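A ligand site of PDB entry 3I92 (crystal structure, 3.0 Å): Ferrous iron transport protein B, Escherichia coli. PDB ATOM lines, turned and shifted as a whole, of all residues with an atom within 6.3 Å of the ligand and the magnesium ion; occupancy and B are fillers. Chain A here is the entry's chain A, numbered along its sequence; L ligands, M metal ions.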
ATOM      1  N   GLY A  10      11.830 -29.711   8.103  1.00  0.00           N
ATOM      2  CA  GLY A  10      11.984 -28.544   7.255  1.00  0.00           C
ATOM      3  C   GLY A  10      11.488 -27.281   7.938  1.00  0.00           C
ATOM      4  O   GLY A  10      11.017 -27.329   9.076  1.00  0.00           O
ATOM      5  N   ASN A  11      11.601 -26.154   7.242  1.00  0.00           N
ATOM      6  CA  ASN A  11      11.102 -24.881   7.755  1.00  0.00           C
ATOM      7  C   ASN A  11       9.583 -24.833   7.680  1.00  0.00           C
ATOM      8  O   ASN A  11       8.963 -25.617   6.960  1.00  0.00           O
ATOM      9  CB  ASN A  11      11.682 -23.724   6.949  1.00  0.00           C
ATOM     10  CG  ASN A  11      13.131 -23.449   7.286  1.00  0.00           C
ATOM     11  OD1 ASN A  11      13.767 -24.211   8.009  1.00  0.00           O
ATOM     12  ND2 ASN A  11      13.653 -22.365   6.766  1.00  0.00           N
ATOM     13  N   PRO A  12       8.970 -23.901   8.437  1.00  0.00           N
ATOM     14  CA  PRO A  12       7.548 -23.664   8.291  1.00  0.00           C
ATOM     15  C   PRO A  12       7.177 -23.344   6.843  1.00  0.00           C
ATOM     16  O   PRO A  12       7.889 -22.608   6.173  1.00  0.00           O
ATOM     17  CB  PRO A  12       7.311 -22.423   9.171  1.00  0.00           C
ATOM     18  CG  PRO A  12       8.410 -22.434  10.150  1.00  0.00           C
ATOM     19  CD  PRO A  12       9.578 -23.047   9.473  1.00  0.00           C
ATOM     20  N   ASN A  13       6.078 -23.929   6.377  1.00  0.00           N
ATOM     21  CA  ASN A  13       5.521 -23.611   5.058  1.00  0.00           C
ATOM     22  C   ASN A  13       6.465 -23.908   3.902  1.00  0.00           C
ATOM     23  O   ASN A  13       6.657 -23.089   3.009  1.00  0.00           O
ATOM     24  CB  ASN A  13       5.082 -22.148   5.024  1.00  0.00           C
ATOM     25  CG  ASN A  13       4.169 -21.848   3.866  1.00  0.00           C
ATOM     26  OD1 ASN A  13       3.009 -22.268   3.853  1.00  0.00           O
ATOM     27  ND2 ASN A  13       4.674 -21.133   2.868  1.00  0.00           N
ATOM     28  N   SER A  14       7.045 -25.106   3.938  1.00  0.00           N
ATOM     29  CA  SER A  14       7.939 -25.564   2.887  1.00  0.00           C
ATOM     30  C   SER A  14       7.337 -26.755   2.139  1.00  0.00           C
ATOM     31  O   SER A  14       8.057 -27.520   1.507  1.00  0.00           O
ATOM     32  CB  SER A  14       9.284 -25.956   3.513  1.00  0.00           C
ATOM     33  OG  SER A  14       9.086 -26.928   4.535  1.00  0.00           O
ATOM     34  N   GLY A  15       6.022 -26.894   2.215  1.00  0.00           N
ATOM     35  CA  GLY A  15       5.303 -27.979   1.542  1.00  0.00           C
ATOM     36  C   GLY A  15       5.497 -29.334   2.194  1.00  0.00           C
ATOM     37  O   GLY A  15       5.470 -30.369   1.530  1.00  0.00           O
ATOM     38  N   LYS A  16       5.666 -29.325   3.513  1.00  0.00           N
ATOM     39  CA  LYS A  16       6.006 -30.532   4.277  1.00  0.00           C
ATOM     40  C   LYS A  16       4.830 -31.504   4.398  1.00  0.00           C
ATOM     41  O   LYS A  16       4.975 -32.690   4.121  1.00  0.00           O
ATOM     42  CB  LYS A  16       6.525 -30.108   5.653  1.00  0.00           C
ATOM     43  CG  LYS A  16       6.967 -31.227   6.578  1.00  0.00           C
ATOM     44  CD  LYS A  16       7.947 -30.730   7.657  1.00  0.00           C
ATOM     45  CE  LYS A  16       7.525 -29.394   8.317  1.00  0.00           C
ATOM     46  NZ  LYS A  16       6.094 -29.359   8.767  1.00  0.00           N
ATOM     47  N   THR A  17       3.661 -30.988   4.779  1.00  0.00           N
ATOM     48  CA  THR A  17       2.473 -31.836   4.971  1.00  0.00           C
ATOM     49  C   THR A  17       1.923 -32.348   3.647  1.00  0.00           C
ATOM     50  O   THR A  17       1.415 -33.467   3.575  1.00  0.00           O
ATOM     51  CB  THR A  17       1.358 -31.094   5.718  1.00  0.00           C
ATOM     52  OG1 THR A  17       1.869 -30.603   6.966  1.00  0.00           O
ATOM     53  CG2 THR A  17       0.190 -32.021   5.993  1.00  0.00           C
ATOM     54  N   THR A  18       1.989 -31.521   2.605  1.00  0.00           N
ATOM     55  CA  THR A  18       1.549 -31.920   1.273  1.00  0.00           C
ATOM     56  C   THR A  18       2.338 -33.136   0.810  1.00  0.00           C
ATOM     57  O   THR A  18       1.790 -34.063   0.218  1.00  0.00           O
ATOM     58  CB  THR A  18       1.717 -30.780   0.256  1.00  0.00           C
ATOM     59  OG1 THR A  18       0.892 -29.677   0.640  1.00  0.00           O
ATOM     60  CG2 THR A  18       1.331 -31.218  -1.151  1.00  0.00           C
ATOM     61  N   LEU A  19       3.642 -33.131   1.101  1.00  0.00           N
ATOM     62  CA  LEU A  19       4.517 -34.253   0.802  1.00  0.00           C
ATOM     63  C   LEU A  19       4.136 -35.478   1.649  1.00  0.00           C
ATOM     64  O   LEU A  19       4.090 -36.610   1.136  1.00  0.00           O
ATOM     65  CB  LEU A  19       5.982 -33.871   1.069  1.00  0.00           C
ATOM     66  CG  LEU A  19       7.077 -34.830   0.588  1.00  0.00           C
ATOM     67  CD1 LEU A  19       6.946 -35.098  -0.903  1.00  0.00           C
ATOM     68  CD2 LEU A  19       8.465 -34.277   0.916  1.00  0.00           C
ATOM     69  N   ASP A  56       5.980 -37.020  10.688  1.00  0.00           N
ATOM     70  CA  ASP A  56       5.860 -35.613  10.268  1.00  0.00           C
ATOM     71  C   ASP A  56       6.248 -34.717  11.434  1.00  0.00           C
ATOM     72  O   ASP A  56       5.459 -34.528  12.361  1.00  0.00           O
ATOM     73  CB  ASP A  56       4.433 -35.296   9.816  1.00  0.00           C
ATOM     74  CG  ASP A  56       4.297 -33.914   9.152  1.00  0.00           C
ATOM     75  OD1 ASP A  56       3.164 -33.564   8.783  1.00  0.00           O
ATOM     76  OD2 ASP A  56       5.314 -33.200   9.017  1.00  0.00           O
ATOM     77  N   LEU A  57       7.467 -34.181  11.387  1.00  0.00           N
ATOM     78  CA  LEU A  57       7.968 -33.327  12.456  1.00  0.00           C
ATOM     79  C   LEU A  57       7.474 -31.908  12.246  1.00  0.00           C
ATOM     80  O   LEU A  57       7.091 -31.540  11.133  1.00  0.00           O
ATOM     81  CB  LEU A  57       9.508 -33.355  12.502  1.00  0.00           C
ATOM     82  CG  LEU A  57      10.139 -34.520  13.272  1.00  0.00           C
ATOM     83  CD1 LEU A  57       9.705 -35.868  12.697  1.00  0.00           C
ATOM     84  CD2 LEU A  57      11.661 -34.420  13.253  1.00  0.00           C
ATOM     85  N   PRO A  58       7.490 -31.083  13.305  1.00  0.00           N
ATOM     86  CA  PRO A  58       7.020 -29.700  13.182  1.00  0.00           C
ATOM     87  C   PRO A  58       8.069 -28.771  12.578  1.00  0.00           C
ATOM     88  O   PRO A  58       9.270 -28.960  12.790  1.00  0.00           O
ATOM     89  CB  PRO A  58       6.719 -29.287  14.631  1.00  0.00           C
ATOM     90  CG  PRO A  58       7.354 -30.319  15.514  1.00  0.00           C
ATOM     91  CD  PRO A  58       7.969 -31.395  14.671  1.00  0.00           C
ATOM     92  N   GLY A  59       7.597 -27.786  11.822  1.00  0.00           N
ATOM     93  CA  GLY A  59       8.476 -26.858  11.123  1.00  0.00           C
ATOM     94  C   GLY A  59       9.363 -26.088  12.075  1.00  0.00           C
ATOM     95  O   GLY A  59       8.914 -25.641  13.130  1.00  0.00           O
ATOM     96  N   ASN A 120      11.876 -28.434  -2.729  1.00  0.00           N
ATOM     97  CA  ASN A 120      10.459 -28.252  -2.996  1.00  0.00           C
ATOM     98  C   ASN A 120      10.092 -26.842  -3.450  1.00  0.00           C
ATOM     99  O   ASN A 120      10.764 -25.861  -3.111  1.00  0.00           O
ATOM    100  CB  ASN A 120       9.664 -28.586  -1.733  1.00  0.00           C
ATOM    101  CG  ASN A 120       8.211 -28.880  -2.014  1.00  0.00           C
ATOM    102  OD1 ASN A 120       7.884 -29.602  -2.955  1.00  0.00           O
ATOM    103  ND2 ASN A 120       7.332 -28.314  -1.204  1.00  0.00           N
ATOM    104  N   MET A 121       9.002 -26.762  -4.216  1.00  0.00           N
ATOM    105  CA  MET A 121       8.417 -25.493  -4.652  1.00  0.00           C
ATOM    106  C   MET A 121       9.294 -24.783  -5.687  1.00  0.00           C
ATOM    107  O   MET A 121       9.424 -23.556  -5.667  1.00  0.00           O
ATOM    108  CB  MET A 121       8.128 -24.578  -3.448  1.00  0.00           C
ATOM    109  CG  MET A 121       7.616 -25.324  -2.217  1.00  0.00           C
ATOM    110  SD  MET A 121       7.146 -24.234  -0.874  1.00  0.00           S
ATOM    111  CE  MET A 121       5.447 -23.891  -1.335  1.00  0.00           C
ATOM    112  N   LEU A 122       9.891 -25.565  -6.592  1.00  0.00           N
ATOM    113  CA  LEU A 122      10.689 -24.992  -7.681  1.00  0.00           C
ATOM    114  C   LEU A 122       9.795 -24.232  -8.660  1.00  0.00           C
ATOM    115  O   LEU A 122      10.278 -23.333  -9.351  1.00  0.00           O
ATOM    116  CB  LEU A 122      11.473 -26.067  -8.443  1.00  0.00           C
ATOM    117  CG  LEU A 122      12.728 -26.594  -7.748  1.00  0.00           C
ATOM    118  CD1 LEU A 122      12.366 -27.814  -6.910  1.00  0.00           C
ATOM    119  CD2 LEU A 122      13.824 -26.943  -8.762  1.00  0.00           C
ATOM    120  N   ASP A 123       8.517 -24.591  -8.731  1.00  0.00           N
ATOM    121  CA  ASP A 123       7.562 -23.847  -9.540  1.00  0.00           C
ATOM    122  C   ASP A 123       7.369 -22.410  -9.047  1.00  0.00           C
ATOM    123  O   ASP A 123       7.074 -21.520  -9.841  1.00  0.00           O
ATOM    124  CB  ASP A 123       6.219 -24.581  -9.577  1.00  0.00           C
ATOM    125  CG  ASP A 123       5.493 -24.521  -8.248  1.00  0.00           C
ATOM    126  OD1 ASP A 123       6.167 -24.484  -7.193  1.00  0.00           O
ATOM    127  OD2 ASP A 123       4.252 -24.502  -8.272  1.00  0.00           O
ATOM    128  N   ILE A 124       7.536 -22.180  -7.750  1.00  0.00           N
ATOM    129  CA  ILE A 124       7.578 -20.826  -7.192  1.00  0.00           C
ATOM    130  C   ILE A 124       8.930 -20.184  -7.481  1.00  0.00           C
ATOM    131  O   ILE A 124       9.012 -19.015  -7.833  1.00  0.00           O
ATOM    132  CB  ILE A 124       7.336 -20.803  -5.666  1.00  0.00           C
ATOM    133  CG1 ILE A 124       5.941 -21.327  -5.333  1.00  0.00           C
ATOM    134  CG2 ILE A 124       7.520 -19.381  -5.119  1.00  0.00           C
ATOM    135  CD1 ILE A 124       5.605 -21.270  -3.857  1.00  0.00           C
ATOM    136  N   LEU A 148      11.465 -31.432  -6.445  1.00  0.00           N
ATOM    137  CA  LEU A 148      10.079 -31.714  -6.117  1.00  0.00           C
ATOM    138  C   LEU A 148       9.126 -30.543  -6.362  1.00  0.00           C
ATOM    139  O   LEU A 148       9.487 -29.375  -6.154  1.00  0.00           O
ATOM    140  CB  LEU A 148       9.955 -32.122  -4.641  1.00  0.00           C
ATOM    141  CG  LEU A 148       9.755 -33.599  -4.312  1.00  0.00           C
ATOM    142  CD1 LEU A 148      11.096 -34.312  -4.189  1.00  0.00           C
ATOM    143  CD2 LEU A 148       8.963 -33.747  -3.039  1.00  0.00           C
ATOM    144  N   VAL A 149       7.913 -30.880  -6.797  1.00  0.00           N
ATOM    145  CA  VAL A 149       6.737 -30.026  -6.639  1.00  0.00           C
ATOM    146  C   VAL A 149       5.690 -30.880  -5.878  1.00  0.00           C
ATOM    147  O   VAL A 149       4.952 -31.656  -6.490  1.00  0.00           O
ATOM    148  CB  VAL A 149       6.183 -29.523  -8.013  1.00  0.00           C
ATOM    149  CG1 VAL A 149       4.893 -28.723  -7.818  1.00  0.00           C
ATOM    150  CG2 VAL A 149       7.224 -28.686  -8.732  1.00  0.00           C
ATOM    151  N   SER A 150       5.672 -30.744  -4.546  1.00  0.00           N
ATOM    152  CA  SER A 150       4.839 -31.590  -3.666  1.00  0.00           C
ATOM    153  C   SER A 150       3.350 -31.552  -4.010  1.00  0.00           C
ATOM    154  O   SER A 150       2.656 -32.583  -3.923  1.00  0.00           O
ATOM    155  CB  SER A 150       5.026 -31.188  -2.204  1.00  0.00           C
ATOM    156  OG  SER A 150       6.379 -31.308  -1.823  1.00  0.00           O
ATOM    157  N   THR A 151       2.860 -30.370  -4.387  1.00  0.00           N
ATOM    158  CA  THR A 151       1.466 -30.185  -4.792  1.00  0.00           C
ATOM    159  C   THR A 151       1.116 -30.940  -6.091  1.00  0.00           C
ATOM    160  O   THR A 151      -0.045 -31.314  -6.300  1.00  0.00           O
ATOM    161  CB  THR A 151       1.116 -28.684  -4.954  1.00  0.00           C
ATOM    162  OG1 THR A 151       2.165 -28.020  -5.684  1.00  0.00           O
ATOM    163  CG2 THR A 151       0.929 -28.020  -3.608  1.00  0.00           C
ATOM    164  N   ARG A 152       2.111 -31.159  -6.945  1.00  0.00           N
ATOM    165  CA  ARG A 152       1.927 -31.850  -8.250  1.00  0.00           C
ATOM    166  C   ARG A 152       2.414 -33.315  -8.258  1.00  0.00           C
ATOM    167  O   ARG A 152       2.143 -34.031  -9.220  1.00  0.00           O
ATOM    168  CB  ARG A 152       2.653 -31.065  -9.353  1.00  0.00           C
ATOM    169  CG  ARG A 152       2.052 -29.706  -9.707  1.00  0.00           C
ATOM    170  CD  ARG A 152       0.746 -29.823 -10.509  1.00  0.00           C
ATOM    171  NE  ARG A 152       0.908 -30.533 -11.785  1.00  0.00           N
ATOM    172  CZ  ARG A 152       0.495 -31.770 -12.045  1.00  0.00           C
ATOM    173  NH1 ARG A 152      -0.127 -32.514 -11.136  1.00  0.00           N
ATOM    174  NH2 ARG A 152       0.714 -32.287 -13.251  1.00  0.00           N
HETATM  175  P1  LIG L   1       3.421 -26.031   8.628  1.00  0.00           P
HETATM  176  O1  LIG L   1       2.934 -24.760   9.268  1.00  0.00           O
HETATM  177  O2  LIG L   1       2.479 -27.192   8.911  1.00  0.00           O
HETATM  178  O3  LIG L   1       4.894 -26.319   8.864  1.00  0.00           O
HETATM  179  C1  LIG L   1       3.238 -25.764   6.838  1.00  0.00           C
HETATM  180  P2  LIG L   1       3.853 -27.180   5.882  1.00  0.00           P
HETATM  181  O4  LIG L   1       5.360 -27.188   6.027  1.00  0.00           O
HETATM  182  O5  LIG L   1       3.155 -28.426   6.342  1.00  0.00           O
HETATM  183  O6  LIG L   1       3.522 -26.940   4.321  1.00  0.00           O
HETATM  184  P3  LIG L   1       2.101 -27.389   3.699  1.00  0.00           P
HETATM  185  O7  LIG L   1       2.336 -28.221   2.467  1.00  0.00           O
HETATM  186  O8  LIG L   1       1.228 -27.960   4.783  1.00  0.00           O
HETATM  187  O9  LIG L   1       1.401 -26.016   3.273  1.00  0.00           O
HETATM  188  C2  LIG L   1       2.100 -24.936   2.653  1.00  0.00           C
HETATM  189  C3  LIG L   1       1.522 -24.646   1.269  1.00  0.00           C
HETATM  190  O10 LIG L   1       2.590 -24.859   0.357  1.00  0.00           O
HETATM  191  C4  LIG L   1       0.354 -25.565   0.836  1.00  0.00           C
HETATM  192  O11 LIG L   1      -0.834 -24.822   0.541  1.00  0.00           O
HETATM  193  C5  LIG L   1       0.808 -26.287  -0.411  1.00  0.00           C
HETATM  194  O12 LIG L   1      -0.174 -26.178  -1.437  1.00  0.00           O
HETATM  195  C6  LIG L   1       2.023 -25.469  -0.802  1.00  0.00           C
HETATM  196  N1  LIG L   1       2.997 -26.168  -1.686  1.00  0.00           N
HETATM  197  C7  LIG L   1       3.761 -27.279  -1.556  1.00  0.00           C
HETATM  198  N2  LIG L   1       4.490 -27.485  -2.706  1.00  0.00           N
HETATM  199  C8  LIG L   1       4.193 -26.473  -3.566  1.00  0.00           C
HETATM  200  C9  LIG L   1       4.561 -26.006  -4.937  1.00  0.00           C
HETATM  201  O13 LIG L   1       5.370 -26.635  -5.637  1.00  0.00           O
HETATM  202  N3  LIG L   1       3.972 -24.877  -5.422  1.00  0.00           N
HETATM  203  C10 LIG L   1       3.081 -24.157  -4.703  1.00  0.00           C
HETATM  204  N4  LIG L   1       2.501 -23.035  -5.197  1.00  0.00           N
HETATM  205  N5  LIG L   1       2.712 -24.525  -3.459  1.00  0.00           N
HETATM  206  C11 LIG L   1       3.218 -25.638  -2.862  1.00  0.00           C
HETATM  207 MG    MG M   1       2.515 -29.162   8.369  1.00  0.00          MG
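NZ of Lys 16 touches the magnesium ion, 3.6 Å away.
Two residues have an atom within 4 Å of the magnesium ion: Lys 16 and Thr 17.
The magnesium ion is bound by an oxygen (O2) of the ligand, the side-chain hydroxyl (OG1) of Thr 17 and an oxygen (O5) of the ligand.
The magnesium ion has three donor atoms within binding distance.
Pro 12 touches the ligand.
Met 121 touches the ligand (CE to C11, 3.2 Å).
Ile 124 touches the ligand.
CG1 of Val 149 touches O13 of the ligand, 3.1 Å away.
Ser 150 touches the ligand.
Hydrophobic or aromatic side chains that line the ligand: Met 121, Ile 124 and Val 149.
Of the 24 residues printed, 14 come within 4 Å of the ligand.
The nearest printed residue that does not touch the ligand is Asn 11 (4.04 Å).
The backbone NH (N) of Thr 17 sits close to an oxygen (O5) of the ligand (3.0 Å).
N of Thr 18 lies within hydrogen-bond range of O7 of the ligand, at 3.3 Å.
The side-chain hydroxyl (OG1) of Thr 18 is in hydrogen-bond range of an oxygen (O7) of the ligand, at 2.7 Å.
N3 of the ligand lies within hydrogen-bond range of OD1 of Asp 123 (2.8 Å).
The side-chain hydroxyl (OG1) of Thr 151 sits close to an oxygen (O13) of the ligand.
O4 of the ligand is in hydrogen-bond range of N of Asn 13, 3.4 Å away.
The backbone NH (N) of Gly 15 lies within hydrogen-bond range of an oxygen (O6) of the ligand (3.3 Å).
N of Lys 16 is in hydrogen-bond range of O6 of the ligand (3.3 Å).
NZ of Lys 16 lies within salt-bridge range of O3 of the ligand (3.3 Å).
ND2 of Asn 120 sits at hydrogen-bond distance from N2 of the ligand, 3.3 Å away.
The backbone NH of Ser 14 is in hydrogen-bond range of an oxygen (O4) of the ligand, 3.4 Å away.
The side-chain amino group (NZ) of Lys 16 lies within salt-bridge range of the side-chain carboxylate (OD2) of Asp 56, 3.9 Å away.
O of Leu 57 sits at hydrogen-bond distance from NZ of Lys 16, 3.4 Å away.
N of Met 121 sits at hydrogen-bond distance from O of Leu 148 (3.3 Å).
The backbone carbonyl oxygen (O) of Ser 14 sits at hydrogen-bond distance from the side-chain amide nitrogen (ND2) of Asn 120, at 2.9 Å.
The side-chain amide oxygen (OD1) of Asn 120 sits at hydrogen-bond distance from the side-chain hydroxyl (OG) of Ser 150 (2.5 Å).
The backbone carbonyl oxygen (O) of Asn 11 sits at hydrogen-bond distance from the side-chain hydroxyl (OG) of Ser 14.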
